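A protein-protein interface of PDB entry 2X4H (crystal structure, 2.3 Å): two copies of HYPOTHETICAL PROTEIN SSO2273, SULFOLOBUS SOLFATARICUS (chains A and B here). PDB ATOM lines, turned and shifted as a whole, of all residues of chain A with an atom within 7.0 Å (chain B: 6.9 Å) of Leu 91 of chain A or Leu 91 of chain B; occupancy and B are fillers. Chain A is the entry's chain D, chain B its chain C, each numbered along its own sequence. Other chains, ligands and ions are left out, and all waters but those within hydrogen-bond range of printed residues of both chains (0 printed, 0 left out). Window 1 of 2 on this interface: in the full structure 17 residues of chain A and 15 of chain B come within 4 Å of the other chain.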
ATOM      1  N   ARG A  86       3.825   5.913 -15.675  1.00  0.00           N
ATOM      2  CA  ARG A  86       4.173   5.122 -14.465  1.00  0.00           C
ATOM      3  C   ARG A  86       5.218   4.042 -14.707  1.00  0.00           C
ATOM      4  O   ARG A  86       6.029   3.750 -13.820  1.00  0.00           O
ATOM      5  CB  ARG A  86       2.905   4.545 -13.816  1.00  0.00           C
ATOM      6  CG  ARG A  86       1.976   5.653 -13.294  1.00  0.00           C
ATOM      7  CD  ARG A  86       0.610   5.144 -12.818  1.00  0.00           C
ATOM      8  NE  ARG A  86      -0.241   6.282 -12.504  1.00  0.00           N
ATOM      9  CZ  ARG A  86      -1.555   6.259 -12.326  1.00  0.00           C
ATOM     10  NH1 ARG A  86      -2.244   5.125 -12.402  1.00  0.00           N
ATOM     11  NH2 ARG A  86      -2.182   7.395 -12.068  1.00  0.00           N
ATOM     12  N   VAL A  87       5.239   3.453 -15.896  1.00  0.00           N
ATOM     13  CA  VAL A  87       6.311   2.511 -16.204  1.00  0.00           C
ATOM     14  C   VAL A  87       7.659   3.254 -16.245  1.00  0.00           C
ATOM     15  O   VAL A  87       8.653   2.744 -15.770  1.00  0.00           O
ATOM     16  CB  VAL A  87       6.080   1.754 -17.530  1.00  0.00           C
ATOM     17  CG1 VAL A  87       7.355   1.005 -17.938  1.00  0.00           C
ATOM     18  CG2 VAL A  87       4.933   0.788 -17.396  1.00  0.00           C
ATOM     19  N   ILE A  88       7.667   4.477 -16.783  1.00  0.00           N
ATOM     20  CA  ILE A  88       8.913   5.229 -16.888  1.00  0.00           C
ATOM     21  C   ILE A  88       9.408   5.620 -15.501  1.00  0.00           C
ATOM     22  O   ILE A  88      10.617   5.571 -15.236  1.00  0.00           O
ATOM     23  CB  ILE A  88       8.757   6.457 -17.817  1.00  0.00           C
ATOM     24  CG1 ILE A  88       8.817   5.984 -19.268  1.00  0.00           C
ATOM     25  CG2 ILE A  88       9.893   7.465 -17.608  1.00  0.00           C
ATOM     26  CD1 ILE A  88       8.146   6.908 -20.221  1.00  0.00           C
ATOM     27  N   GLU A  89       8.472   5.970 -14.617  1.00  0.00           N
ATOM     28  CA  GLU A  89       8.812   6.378 -13.249  1.00  0.00           C
ATOM     29  C   GLU A  89       9.529   5.313 -12.487  1.00  0.00           C
ATOM     30  O   GLU A  89      10.426   5.618 -11.695  1.00  0.00           O
ATOM     31  CB  GLU A  89       7.578   6.702 -12.435  1.00  0.00           C
ATOM     32  CG  GLU A  89       6.936   7.962 -12.809  1.00  0.00           C
ATOM     33  CD  GLU A  89       5.886   8.383 -11.816  1.00  0.00           C
ATOM     34  OE1 GLU A  89       5.075   7.571 -11.398  1.00  0.00           O
ATOM     35  OE2 GLU A  89       5.872   9.549 -11.449  1.00  0.00           O
ATOM     36  N   ILE A  90       9.103   4.067 -12.676  1.00  0.00           N
ATOM     37  CA  ILE A  90       9.748   2.936 -11.984  1.00  0.00           C
ATOM     38  C   ILE A  90      11.200   2.814 -12.453  1.00  0.00           C
ATOM     39  O   ILE A  90      12.118   2.660 -11.624  1.00  0.00           O
ATOM     40  CB  ILE A  90       9.006   1.629 -12.205  1.00  0.00           C
ATOM     41  CG1 ILE A  90       7.617   1.700 -11.554  1.00  0.00           C
ATOM     42  CG2 ILE A  90       9.789   0.418 -11.611  1.00  0.00           C
ATOM     43  CD1 ILE A  90       6.795   0.435 -11.694  1.00  0.00           C
ATOM     44  N   LEU A  91      11.414   2.904 -13.771  1.00  0.00           N
ATOM     45  CA  LEU A  91      12.782   2.869 -14.321  1.00  0.00           C
ATOM     46  C   LEU A  91      13.617   3.956 -13.692  1.00  0.00           C
ATOM     47  O   LEU A  91      14.772   3.731 -13.317  1.00  0.00           O
ATOM     48  CB  LEU A  91      12.770   3.054 -15.836  1.00  0.00           C
ATOM     49  CG  LEU A  91      14.144   3.175 -16.505  1.00  0.00           C
ATOM     50  CD1 LEU A  91      14.965   1.910 -16.260  1.00  0.00           C
ATOM     51  CD2 LEU A  91      13.988   3.472 -18.000  1.00  0.00           C
ATOM     52  N   LEU A  92      13.031   5.144 -13.564  1.00  0.00           N
ATOM     53  CA  LEU A  92      13.785   6.313 -13.095  1.00  0.00           C
ATOM     54  C   LEU A  92      14.098   6.155 -11.628  1.00  0.00           C
ATOM     55  O   LEU A  92      15.230   6.370 -11.217  1.00  0.00           O
ATOM     56  CB  LEU A  92      13.042   7.621 -13.360  1.00  0.00           C
ATOM     57  CG  LEU A  92      12.784   7.959 -14.829  1.00  0.00           C
ATOM     58  CD1 LEU A  92      12.263   9.420 -14.967  1.00  0.00           C
ATOM     59  CD2 LEU A  92      14.066   7.717 -15.661  1.00  0.00           C
ATOM     60  N   VAL A  93      13.134   5.697 -10.842  1.00  0.00           N
ATOM     61  CA  VAL A  93      13.425   5.438  -9.442  1.00  0.00           C
ATOM     62  C   VAL A  93      14.425   4.292  -9.336  1.00  0.00           C
ATOM     63  O   VAL A  93      15.248   4.294  -8.431  1.00  0.00           O
ATOM     64  CB  VAL A  93      12.159   5.176  -8.605  1.00  0.00           C
ATOM     65  CG1 VAL A  93      12.517   4.745  -7.173  1.00  0.00           C
ATOM     66  CG2 VAL A  93      11.274   6.464  -8.585  1.00  0.00           C
ATOM     67  N   ASN A  94      14.403   3.343 -10.270  1.00  0.00           N
ATOM     68  CA  ASN A  94      15.338   2.213 -10.196  1.00  0.00           C
ATOM     69  C   ASN A  94      16.776   2.642 -10.415  1.00  0.00           C
ATOM     70  O   ASN A  94      17.701   2.014  -9.888  1.00  0.00           O
ATOM     71  CB  ASN A  94      14.989   1.103 -11.203  1.00  0.00           C
ATOM     72  CG  ASN A  94      13.886   0.240 -10.724  1.00  0.00           C
ATOM     73  OD1 ASN A  94      13.332   0.505  -9.662  1.00  0.00           O
ATOM     74  ND2 ASN A  94      13.560  -0.822 -11.472  1.00  0.00           N
ATOM     75  N   ILE A  95      16.962   3.704 -11.195  1.00  0.00           N
ATOM     76  CA  ILE A  95      18.303   4.181 -11.462  1.00  0.00           C
ATOM     77  C   ILE A  95      18.792   5.214 -10.443  1.00  0.00           C
ATOM     78  O   ILE A  95      19.905   5.694 -10.571  1.00  0.00           O
ATOM     79  CB  ILE A  95      18.458   4.683 -12.915  1.00  0.00           C
ATOM     80  CG1 ILE A  95      17.750   6.020 -13.137  1.00  0.00           C
ATOM     81  CG2 ILE A  95      17.982   3.607 -13.898  1.00  0.00           C
ATOM     82  CD1 ILE A  95      17.957   6.591 -14.538  1.00  0.00           C
ATOM     83  N   GLY A  96      17.985   5.548  -9.437  1.00  0.00           N
ATOM     84  CA  GLY A  96      18.422   6.449  -8.337  1.00  0.00           C
ATOM     85  C   GLY A  96      17.814   7.857  -8.339  1.00  0.00           C
ATOM     86  O   GLY A  96      18.219   8.715  -7.566  1.00  0.00           O
ATOM     87  N   ILE A  97      16.815   8.101  -9.175  1.00  0.00           N
ATOM     88  CA  ILE A  97      16.175   9.407  -9.206  1.00  0.00           C
ATOM     89  C   ILE A  97      15.076   9.500  -8.156  1.00  0.00           C
ATOM     90  O   ILE A  97      14.243   8.606  -8.061  1.00  0.00           O
ATOM     91  CB  ILE A  97      15.611   9.684 -10.588  1.00  0.00           C
ATOM     92  CG1 ILE A  97      16.765   9.996 -11.527  1.00  0.00           C
ATOM     93  CG2 ILE A  97      14.609  10.861 -10.572  1.00  0.00           C
ATOM     94  CD1 ILE A  97      16.455   9.713 -12.964  1.00  0.00           C
ATOM     95  N   ALA A 102      11.288  12.084 -10.474  1.00  0.00           N
ATOM     96  CA  ALA A 102      10.964  11.104 -11.509  1.00  0.00           C
ATOM     97  C   ALA A 102       9.590  11.360 -12.138  1.00  0.00           C
ATOM     98  O   ALA A 102       9.433  11.210 -13.338  1.00  0.00           O
ATOM     99  CB  ALA A 102      11.047   9.699 -10.944  1.00  0.00           C
ATOM    100  N   ILE A 117       8.792   0.317 -26.712  1.00  0.00           N
ATOM    101  CA  ILE A 117       9.725   0.482 -25.603  1.00  0.00           C
ATOM    102  C   ILE A 117       9.004   0.371 -24.280  1.00  0.00           C
ATOM    103  O   ILE A 117       9.478  -0.329 -23.363  1.00  0.00           O
ATOM    104  CB  ILE A 117      10.502   1.821 -25.657  1.00  0.00           C
ATOM    105  CG1 ILE A 117      11.445   1.816 -26.852  1.00  0.00           C
ATOM    106  CG2 ILE A 117      11.281   2.059 -24.365  1.00  0.00           C
ATOM    107  CD1 ILE A 117      12.021   3.155 -27.173  1.00  0.00           C
ATOM    108  N   LEU A 121       9.811  -2.442 -21.561  1.00  0.00           N
ATOM    109  CA  LEU A 121      10.200  -1.930 -20.241  1.00  0.00           C
ATOM    110  C   LEU A 121       9.332  -2.547 -19.164  1.00  0.00           C
ATOM    111  O   LEU A 121       9.838  -2.934 -18.116  1.00  0.00           O
ATOM    112  CB  LEU A 121      10.089  -0.397 -20.160  1.00  0.00           C
ATOM    113  CG  LEU A 121      11.274   0.425 -20.663  1.00  0.00           C
ATOM    114  CD1 LEU A 121      10.927   1.882 -20.592  1.00  0.00           C
ATOM    115  CD2 LEU A 121      12.587   0.162 -19.893  1.00  0.00           C
ATOM    116  N   TYR A 124      10.477  -5.980 -18.695  1.00  0.00           N
ATOM    117  CA  TYR A 124      11.766  -5.894 -18.070  1.00  0.00           C
ATOM    118  C   TYR A 124      11.671  -5.519 -16.591  1.00  0.00           C
ATOM    119  O   TYR A 124      12.482  -5.980 -15.775  1.00  0.00           O
ATOM    120  CB  TYR A 124      12.597  -4.884 -18.834  1.00  0.00           C
ATOM    121  CG  TYR A 124      13.862  -4.432 -18.153  1.00  0.00           C
ATOM    122  CD1 TYR A 124      14.917  -5.305 -17.940  1.00  0.00           C
ATOM    123  CD2 TYR A 124      14.016  -3.109 -17.767  1.00  0.00           C
ATOM    124  CE1 TYR A 124      16.083  -4.872 -17.329  1.00  0.00           C
ATOM    125  CE2 TYR A 124      15.183  -2.664 -17.162  1.00  0.00           C
ATOM    126  CZ  TYR A 124      16.208  -3.543 -16.938  1.00  0.00           C
ATOM    127  OH  TYR A 124      17.355  -3.054 -16.337  1.00  0.00           O
ATOM    128  N   LEU A 125      10.678  -4.698 -16.239  1.00  0.00           N
ATOM    129  CA  LEU A 125      10.521  -4.262 -14.850  1.00  0.00           C
ATOM    130  C   LEU A 125       9.749  -5.245 -13.976  1.00  0.00           C
ATOM    131  O   LEU A 125       9.666  -5.041 -12.767  1.00  0.00           O
ATOM    132  CB  LEU A 125       9.858  -2.878 -14.779  1.00  0.00           C
ATOM    133  CG  LEU A 125      10.719  -1.746 -15.325  1.00  0.00           C
ATOM    134  CD1 LEU A 125       9.935  -0.444 -15.324  1.00  0.00           C
ATOM    135  CD2 LEU A 125      12.004  -1.626 -14.532  1.00  0.00           C
ATOM    136  N   PRO A 132       5.915   4.079  -8.251  1.00  0.00           N
ATOM    137  CA  PRO A 132       6.516   4.355  -6.947  1.00  0.00           C
ATOM    138  C   PRO A 132       5.616   5.109  -5.948  1.00  0.00           C
ATOM    139  O   PRO A 132       5.868   5.018  -4.746  1.00  0.00           O
ATOM    140  CB  PRO A 132       7.734   5.223  -7.301  1.00  0.00           C
ATOM    141  CG  PRO A 132       8.047   4.903  -8.691  1.00  0.00           C
ATOM    142  CD  PRO A 132       6.729   4.648  -9.340  1.00  0.00           C
ATOM    143  N   ARG B  86      23.464   7.198 -27.094  1.00  0.00           N
ATOM    144  CA  ARG B  86      24.171   5.934 -27.009  1.00  0.00           C
ATOM    145  C   ARG B  86      23.896   5.159 -25.703  1.00  0.00           C
ATOM    146  O   ARG B  86      23.800   3.918 -25.713  1.00  0.00           O
ATOM    147  CB  ARG B  86      25.664   6.215 -27.232  1.00  0.00           C
ATOM    148  CG  ARG B  86      25.949   6.635 -28.662  1.00  0.00           C
ATOM    149  CD  ARG B  86      27.393   7.035 -28.943  1.00  0.00           C
ATOM    150  NE  ARG B  86      27.508   7.462 -30.336  1.00  0.00           N
ATOM    151  CZ  ARG B  86      28.568   8.038 -30.900  1.00  0.00           C
ATOM    152  NH1 ARG B  86      29.660   8.328 -30.218  1.00  0.00           N
ATOM    153  NH2 ARG B  86      28.506   8.385 -32.170  1.00  0.00           N
ATOM    154  N   VAL B  87      23.746   5.867 -24.587  1.00  0.00           N
ATOM    155  CA  VAL B  87      23.302   5.225 -23.358  1.00  0.00           C
ATOM    156  C   VAL B  87      21.893   4.633 -23.525  1.00  0.00           C
ATOM    157  O   VAL B  87      21.655   3.488 -23.143  1.00  0.00           O
ATOM    158  CB  VAL B  87      23.366   6.193 -22.167  1.00  0.00           C
ATOM    159  CG1 VAL B  87      22.668   5.603 -20.945  1.00  0.00           C
ATOM    160  CG2 VAL B  87      24.837   6.562 -21.865  1.00  0.00           C
ATOM    161  N   ILE B  88      20.963   5.388 -24.107  1.00  0.00           N
ATOM    162  CA  ILE B  88      19.634   4.847 -24.395  1.00  0.00           C
ATOM    163  C   ILE B  88      19.725   3.618 -25.306  1.00  0.00           C
ATOM    164  O   ILE B  88      19.083   2.612 -25.031  1.00  0.00           O
ATOM    165  CB  ILE B  88      18.692   5.908 -24.994  1.00  0.00           C
ATOM    166  CG1 ILE B  88      18.136   6.803 -23.885  1.00  0.00           C
ATOM    167  CG2 ILE B  88      17.494   5.241 -25.688  1.00  0.00           C
ATOM    168  CD1 ILE B  88      17.593   8.101 -24.386  1.00  0.00           C
ATOM    169  N   GLU B  89      20.551   3.668 -26.349  1.00  0.00           N
ATOM    170  CA  GLU B  89      20.689   2.520 -27.232  1.00  0.00           C
ATOM    171  C   GLU B  89      21.029   1.250 -26.473  1.00  0.00           C
ATOM    172  O   GLU B  89      20.495   0.193 -26.778  1.00  0.00           O
ATOM    173  CB  GLU B  89      21.795   2.714 -28.264  1.00  0.00           C
ATOM    174  CG  GLU B  89      21.486   3.684 -29.326  1.00  0.00           C
ATOM    175  CD  GLU B  89      22.384   3.537 -30.545  1.00  0.00           C
ATOM    176  OE1 GLU B  89      23.597   3.199 -30.398  1.00  0.00           O
ATOM    177  OE2 GLU B  89      21.866   3.819 -31.655  1.00  0.00           O
ATOM    178  N   ILE B  90      21.959   1.359 -25.525  1.00  0.00           N
ATOM    179  CA  ILE B  90      22.394   0.225 -24.734  1.00  0.00           C
ATOM    180  C   ILE B  90      21.257  -0.342 -23.907  1.00  0.00           C
ATOM    181  O   ILE B  90      21.083  -1.568 -23.859  1.00  0.00           O
ATOM    182  CB  ILE B  90      23.593   0.555 -23.823  1.00  0.00           C
ATOM    183  CG1 ILE B  90      24.862   0.688 -24.673  1.00  0.00           C
ATOM    184  CG2 ILE B  90      23.819  -0.562 -22.758  1.00  0.00           C
ATOM    185  CD1 ILE B  90      26.082   1.180 -23.934  1.00  0.00           C
ATOM    186  N   LEU B  91      20.492   0.539 -23.256  1.00  0.00           N
ATOM    187  CA  LEU B  91      19.305   0.104 -22.505  1.00  0.00           C
ATOM    188  C   LEU B  91      18.378  -0.660 -23.435  1.00  0.00           C
ATOM    189  O   LEU B  91      17.885  -1.720 -23.071  1.00  0.00           O
ATOM    190  CB  LEU B  91      18.554   1.280 -21.856  1.00  0.00           C
ATOM    191  CG  LEU B  91      17.184   0.958 -21.239  1.00  0.00           C
ATOM    192  CD1 LEU B  91      17.323   0.004 -20.073  1.00  0.00           C
ATOM    193  CD2 LEU B  91      16.444   2.280 -20.844  1.00  0.00           C
ATOM    194  N   LEU B  92      18.164  -0.141 -24.636  1.00  0.00           N
ATOM    195  CA  LEU B  92      17.168  -0.706 -25.539  1.00  0.00           C
ATOM    196  C   LEU B  92      17.606  -2.067 -26.060  1.00  0.00           C
ATOM    197  O   LEU B  92      16.806  -3.017 -26.110  1.00  0.00           O
ATOM    198  CB  LEU B  92      16.842   0.271 -26.673  1.00  0.00           C
ATOM    199  CG  LEU B  92      16.198   1.594 -26.243  1.00  0.00           C
ATOM    200  CD1 LEU B  92      15.799   2.406 -27.448  1.00  0.00           C
ATOM    201  CD2 LEU B  92      14.987   1.385 -25.327  1.00  0.00           C
ATOM    202  N   VAL B  93      18.892  -2.205 -26.373  1.00  0.00           N
ATOM    203  CA  VAL B  93      19.405  -3.505 -26.791  1.00  0.00           C
ATOM    204  C   VAL B  93      19.337  -4.477 -25.617  1.00  0.00           C
ATOM    205  O   VAL B  93      18.980  -5.653 -25.805  1.00  0.00           O
ATOM    206  CB  VAL B  93      20.823  -3.387 -27.403  1.00  0.00           C
ATOM    207  CG1 VAL B  93      21.517  -4.745 -27.529  1.00  0.00           C
ATOM    208  CG2 VAL B  93      20.748  -2.693 -28.767  1.00  0.00           C
ATOM    209  N   ASN B  94      19.654  -4.012 -24.406  1.00  0.00           N
ATOM    210  CA  ASN B  94      19.715  -4.934 -23.236  1.00  0.00           C
ATOM    211  C   ASN B  94      18.319  -5.430 -22.841  1.00  0.00           C
ATOM    212  O   ASN B  94      18.183  -6.491 -22.204  1.00  0.00           O
ATOM    213  CB  ASN B  94      20.364  -4.290 -22.010  1.00  0.00           C
ATOM    214  CG  ASN B  94      21.844  -4.079 -22.162  1.00  0.00           C
ATOM    215  OD1 ASN B  94      22.453  -4.403 -23.201  1.00  0.00           O
ATOM    216  ND2 ASN B  94      22.458  -3.517 -21.109  1.00  0.00           N
ATOM    217  N   ILE B  95      17.282  -4.672 -23.211  1.00  0.00           N
ATOM    218  CA  ILE B  95      15.917  -5.120 -22.936  1.00  0.00           C
ATOM    219  C   ILE B  95      15.280  -5.772 -24.143  1.00  0.00           C
ATOM    220  O   ILE B  95      14.079  -6.001 -24.138  1.00  0.00           O
ATOM    221  CB  ILE B  95      15.023  -3.977 -22.389  1.00  0.00           C
ATOM    222  CG1 ILE B  95      14.635  -2.974 -23.478  1.00  0.00           C
ATOM    223  CG2 ILE B  95      15.736  -3.231 -21.259  1.00  0.00           C
ATOM    224  CD1 ILE B  95      13.777  -1.823 -22.960  1.00  0.00           C
ATOM    225  N   GLY B  96      16.064  -6.069 -25.175  1.00  0.00           N
ATOM    226  CA  GLY B  96      15.598  -6.912 -26.282  1.00  0.00           C
ATOM    227  C   GLY B  96      15.238  -6.267 -27.610  1.00  0.00           C
ATOM    228  O   GLY B  96      14.674  -6.915 -28.465  1.00  0.00           O
ATOM    229  N   ILE B  97      15.552  -4.995 -27.802  1.00  0.00           N
ATOM    230  CA  ILE B  97      15.272  -4.317 -29.078  1.00  0.00           C
ATOM    231  C   ILE B  97      16.502  -4.395 -30.014  1.00  0.00           C
ATOM    232  O   ILE B  97      17.609  -4.089 -29.602  1.00  0.00           O
ATOM    233  CB  ILE B  97      14.840  -2.844 -28.826  1.00  0.00           C
ATOM    234  CG1 ILE B  97      13.544  -2.836 -28.006  1.00  0.00           C
ATOM    235  CG2 ILE B  97      14.578  -2.131 -30.135  1.00  0.00           C
ATOM    236  CD1 ILE B  97      13.101  -1.537 -27.483  1.00  0.00           C
ATOM    237  N   ILE B 117      19.009  12.025 -15.638  1.00  0.00           N
ATOM    238  CA  ILE B 117      18.582  10.696 -16.065  1.00  0.00           C
ATOM    239  C   ILE B 117      19.669   9.998 -16.864  1.00  0.00           C
ATOM    240  O   ILE B 117      20.006   8.822 -16.611  1.00  0.00           O
ATOM    241  CB  ILE B 117      17.282  10.746 -16.900  1.00  0.00           C
ATOM    242  CG1 ILE B 117      16.094  11.120 -16.025  1.00  0.00           C
ATOM    243  CG2 ILE B 117      17.001   9.421 -17.542  1.00  0.00           C
ATOM    244  CD1 ILE B 117      14.815  11.410 -16.808  1.00  0.00           C
ATOM    245  N   LEU B 121      21.546   6.740 -15.665  1.00  0.00           N
ATOM    246  CA  LEU B 121      21.317   5.565 -16.487  1.00  0.00           C
ATOM    247  C   LEU B 121      22.664   5.018 -16.934  1.00  0.00           C
ATOM    248  O   LEU B 121      22.859   3.810 -16.995  1.00  0.00           O
ATOM    249  CB  LEU B 121      20.397   5.861 -17.678  1.00  0.00           C
ATOM    250  CG  LEU B 121      20.043   4.709 -18.633  1.00  0.00           C
ATOM    251  CD1 LEU B 121      19.390   3.542 -17.891  1.00  0.00           C
ATOM    252  CD2 LEU B 121      19.173   5.155 -19.784  1.00  0.00           C
ATOM    253  N   TYR B 124      23.952   3.149 -13.982  1.00  0.00           N
ATOM    254  CA  TYR B 124      23.157   1.922 -13.830  1.00  0.00           C
ATOM    255  C   TYR B 124      23.563   0.834 -14.821  1.00  0.00           C
ATOM    256  O   TYR B 124      23.550  -0.333 -14.470  1.00  0.00           O
ATOM    257  CB  TYR B 124      21.700   2.272 -14.003  1.00  0.00           C
ATOM    258  CG  TYR B 124      20.704   1.167 -13.844  1.00  0.00           C
ATOM    259  CD1 TYR B 124      20.289   0.759 -12.577  1.00  0.00           C
ATOM    260  CD2 TYR B 124      20.109   0.580 -14.965  1.00  0.00           C
ATOM    261  CE1 TYR B 124      19.327  -0.258 -12.426  1.00  0.00           C
ATOM    262  CE2 TYR B 124      19.145  -0.417 -14.834  1.00  0.00           C
ATOM    263  CZ  TYR B 124      18.766  -0.835 -13.558  1.00  0.00           C
ATOM    264  OH  TYR B 124      17.830  -1.828 -13.421  1.00  0.00           O
ATOM    265  N   LEU B 125      23.942   1.229 -16.040  1.00  0.00           N
ATOM    266  CA  LEU B 125      24.370   0.286 -17.084  1.00  0.00           C
ATOM    267  C   LEU B 125      25.844  -0.067 -17.005  1.00  0.00           C
ATOM    268  O   LEU B 125      26.370  -0.742 -17.884  1.00  0.00           O
ATOM    269  CB  LEU B 125      24.082   0.869 -18.461  1.00  0.00           C
ATOM    270  CG  LEU B 125      22.600   1.144 -18.770  1.00  0.00           C
ATOM    271  CD1 LEU B 125      22.475   1.982 -20.086  1.00  0.00           C
ATOM    272  CD2 LEU B 125      21.776  -0.130 -18.845  1.00  0.00           C
ATOM    273  N   PRO B 132      26.286   0.046 -29.180  1.00  0.00           N
ATOM    274  CA  PRO B 132      26.288  -1.213 -29.946  1.00  0.00           C
ATOM    275  C   PRO B 132      26.781  -1.094 -31.407  1.00  0.00           C
ATOM    276  O   PRO B 132      27.028  -2.117 -32.039  1.00  0.00           O
ATOM    277  CB  PRO B 132      24.826  -1.633 -29.932  1.00  0.00           C
ATOM    278  CG  PRO B 132      24.196  -0.829 -28.847  1.00  0.00           C
ATOM    279  CD  PRO B 132      24.913   0.463 -28.857  1.00  0.00           C
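The side-chain hydroxyl (OH) of Tyr 124 of chain B sits at hydrogen-bond distance from the side-chain hydroxyl (OH) of Tyr 124 of chain A (3.2 Å).
N of Ile 97 of chain B sits at hydrogen-bond distance from O of Leu 92 of chain B, 2.9 Å away.
N of Ile 97 of chain A is in hydrogen-bond range of O of Leu 92 of chain A, at 3.1 Å.
The backbone carbonyl oxygen (O) of Ile 90 of chain A lies close to the side-chain amide oxygen (OD1) of Asn 94 of chain A, at 3.2 Å.
Among the printed residues, merely in contact across the chains: Leu 91 of chain A with Leu 91 of chain B (3.9 Å), Leu 92 of chain A with Ile 117 of chain B (3.7 Å), Asn 94 of chain A with Tyr 124 of chain B (3.8 Å), Ile 95 of chain A with Ile 117 of chain B (3.7 Å), Ile 95 of chain A with Leu 121 of chain B (3.8 Å), Ile 95 of chain A with Tyr 124 of chain B (3.7 Å), Ile 97 of chain A with Ile 117 of chain B (3.4 Å), Ile 117 of chain A with Leu 92 of chain B (3.9 Å), Ile 117 of chain A with Ile 97 of chain B (3.8 Å), Leu 121 of chain A with Ile 95 of chain B (3.8 Å) and Tyr 124 of chain A with Ile 95 of chain B (3.8 Å).
Leu 91 of chain A touches just one residue of chain B: Leu 91.
Printed residues of chain A within 4 Å of Leu 91 of chain B: Leu 91.
Printed residues of chain A within 4 Å of Tyr 124 of chain B: Asn 94, Ile 95 and Tyr 124.
Of the printed residues of chain B, Leu 121 of chain A touches Ile 95.
Of the printed residues of chain A, Ile 117 of chain B touches Leu 92, Ile 95 and Ile 97.
Of the printed residues of chain A, Ile 95 of chain B touches Leu 121 (3.8 Å) and Tyr 124 (3.8 Å).
Of the printed residues of chain B, Tyr 124 of chain A touches Ile 95 (3.8 Å) and Tyr 124 (3.2 Å).
The nearest printed residue of chain A that does not touch Leu 91 of chain B is Tyr 124 of chain A (4.5 Å).
Of the 17 printed residues of chain B, 7 touch a printed residue of chain A.
Printed residues of chain B that touch a printed residue of chain A: Leu 91, Leu 92, Ile 95, Ile 97, Ile 117, Leu 121 and Tyr 124.
Hydrophobic or aromatic side chains of chain B within 4 Å of the printed part of chain A: Leu 91, Leu 92, Ile 95, Ile 97, Ile 117 and Tyr 124.
Printed residues of chain A that touch a printed residue of chain B: Leu 91, Leu 92, Asn 94, Ile 95, Ile 97, Ile 117, Leu 121 and Tyr 124.
Among the printed residues, 12 pairs touch across the chains.
Asn 94 of chain A touches Tyr 124 of chain B, but with the chains exchanged Tyr 124 of chain A does not touch Asn 94 of chain B (5.5 Å).
Ile 95 of chain A touches Tyr 124 of chain B, and with the chains exchanged Tyr 124 of chain A touches Ile 95 of chain B.
Ile 97 of chain A touches Ile 117 of chain B, and with the chains exchanged Ile 117 of chain A touches Ile 97 of chain B.
Tyr 124 of chain B touches its own counterpart, Tyr 124 of chain A.
Positions printed for both chains: 86, 87, 88, 89, 90, 91, 92, 93, 94, 95, 96, 97, 117, 121, 124, 125 and 132.
Of the 12 pairs that touch across the chains among the printed residues, 10 have their exchanged pair printed and touching as well.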
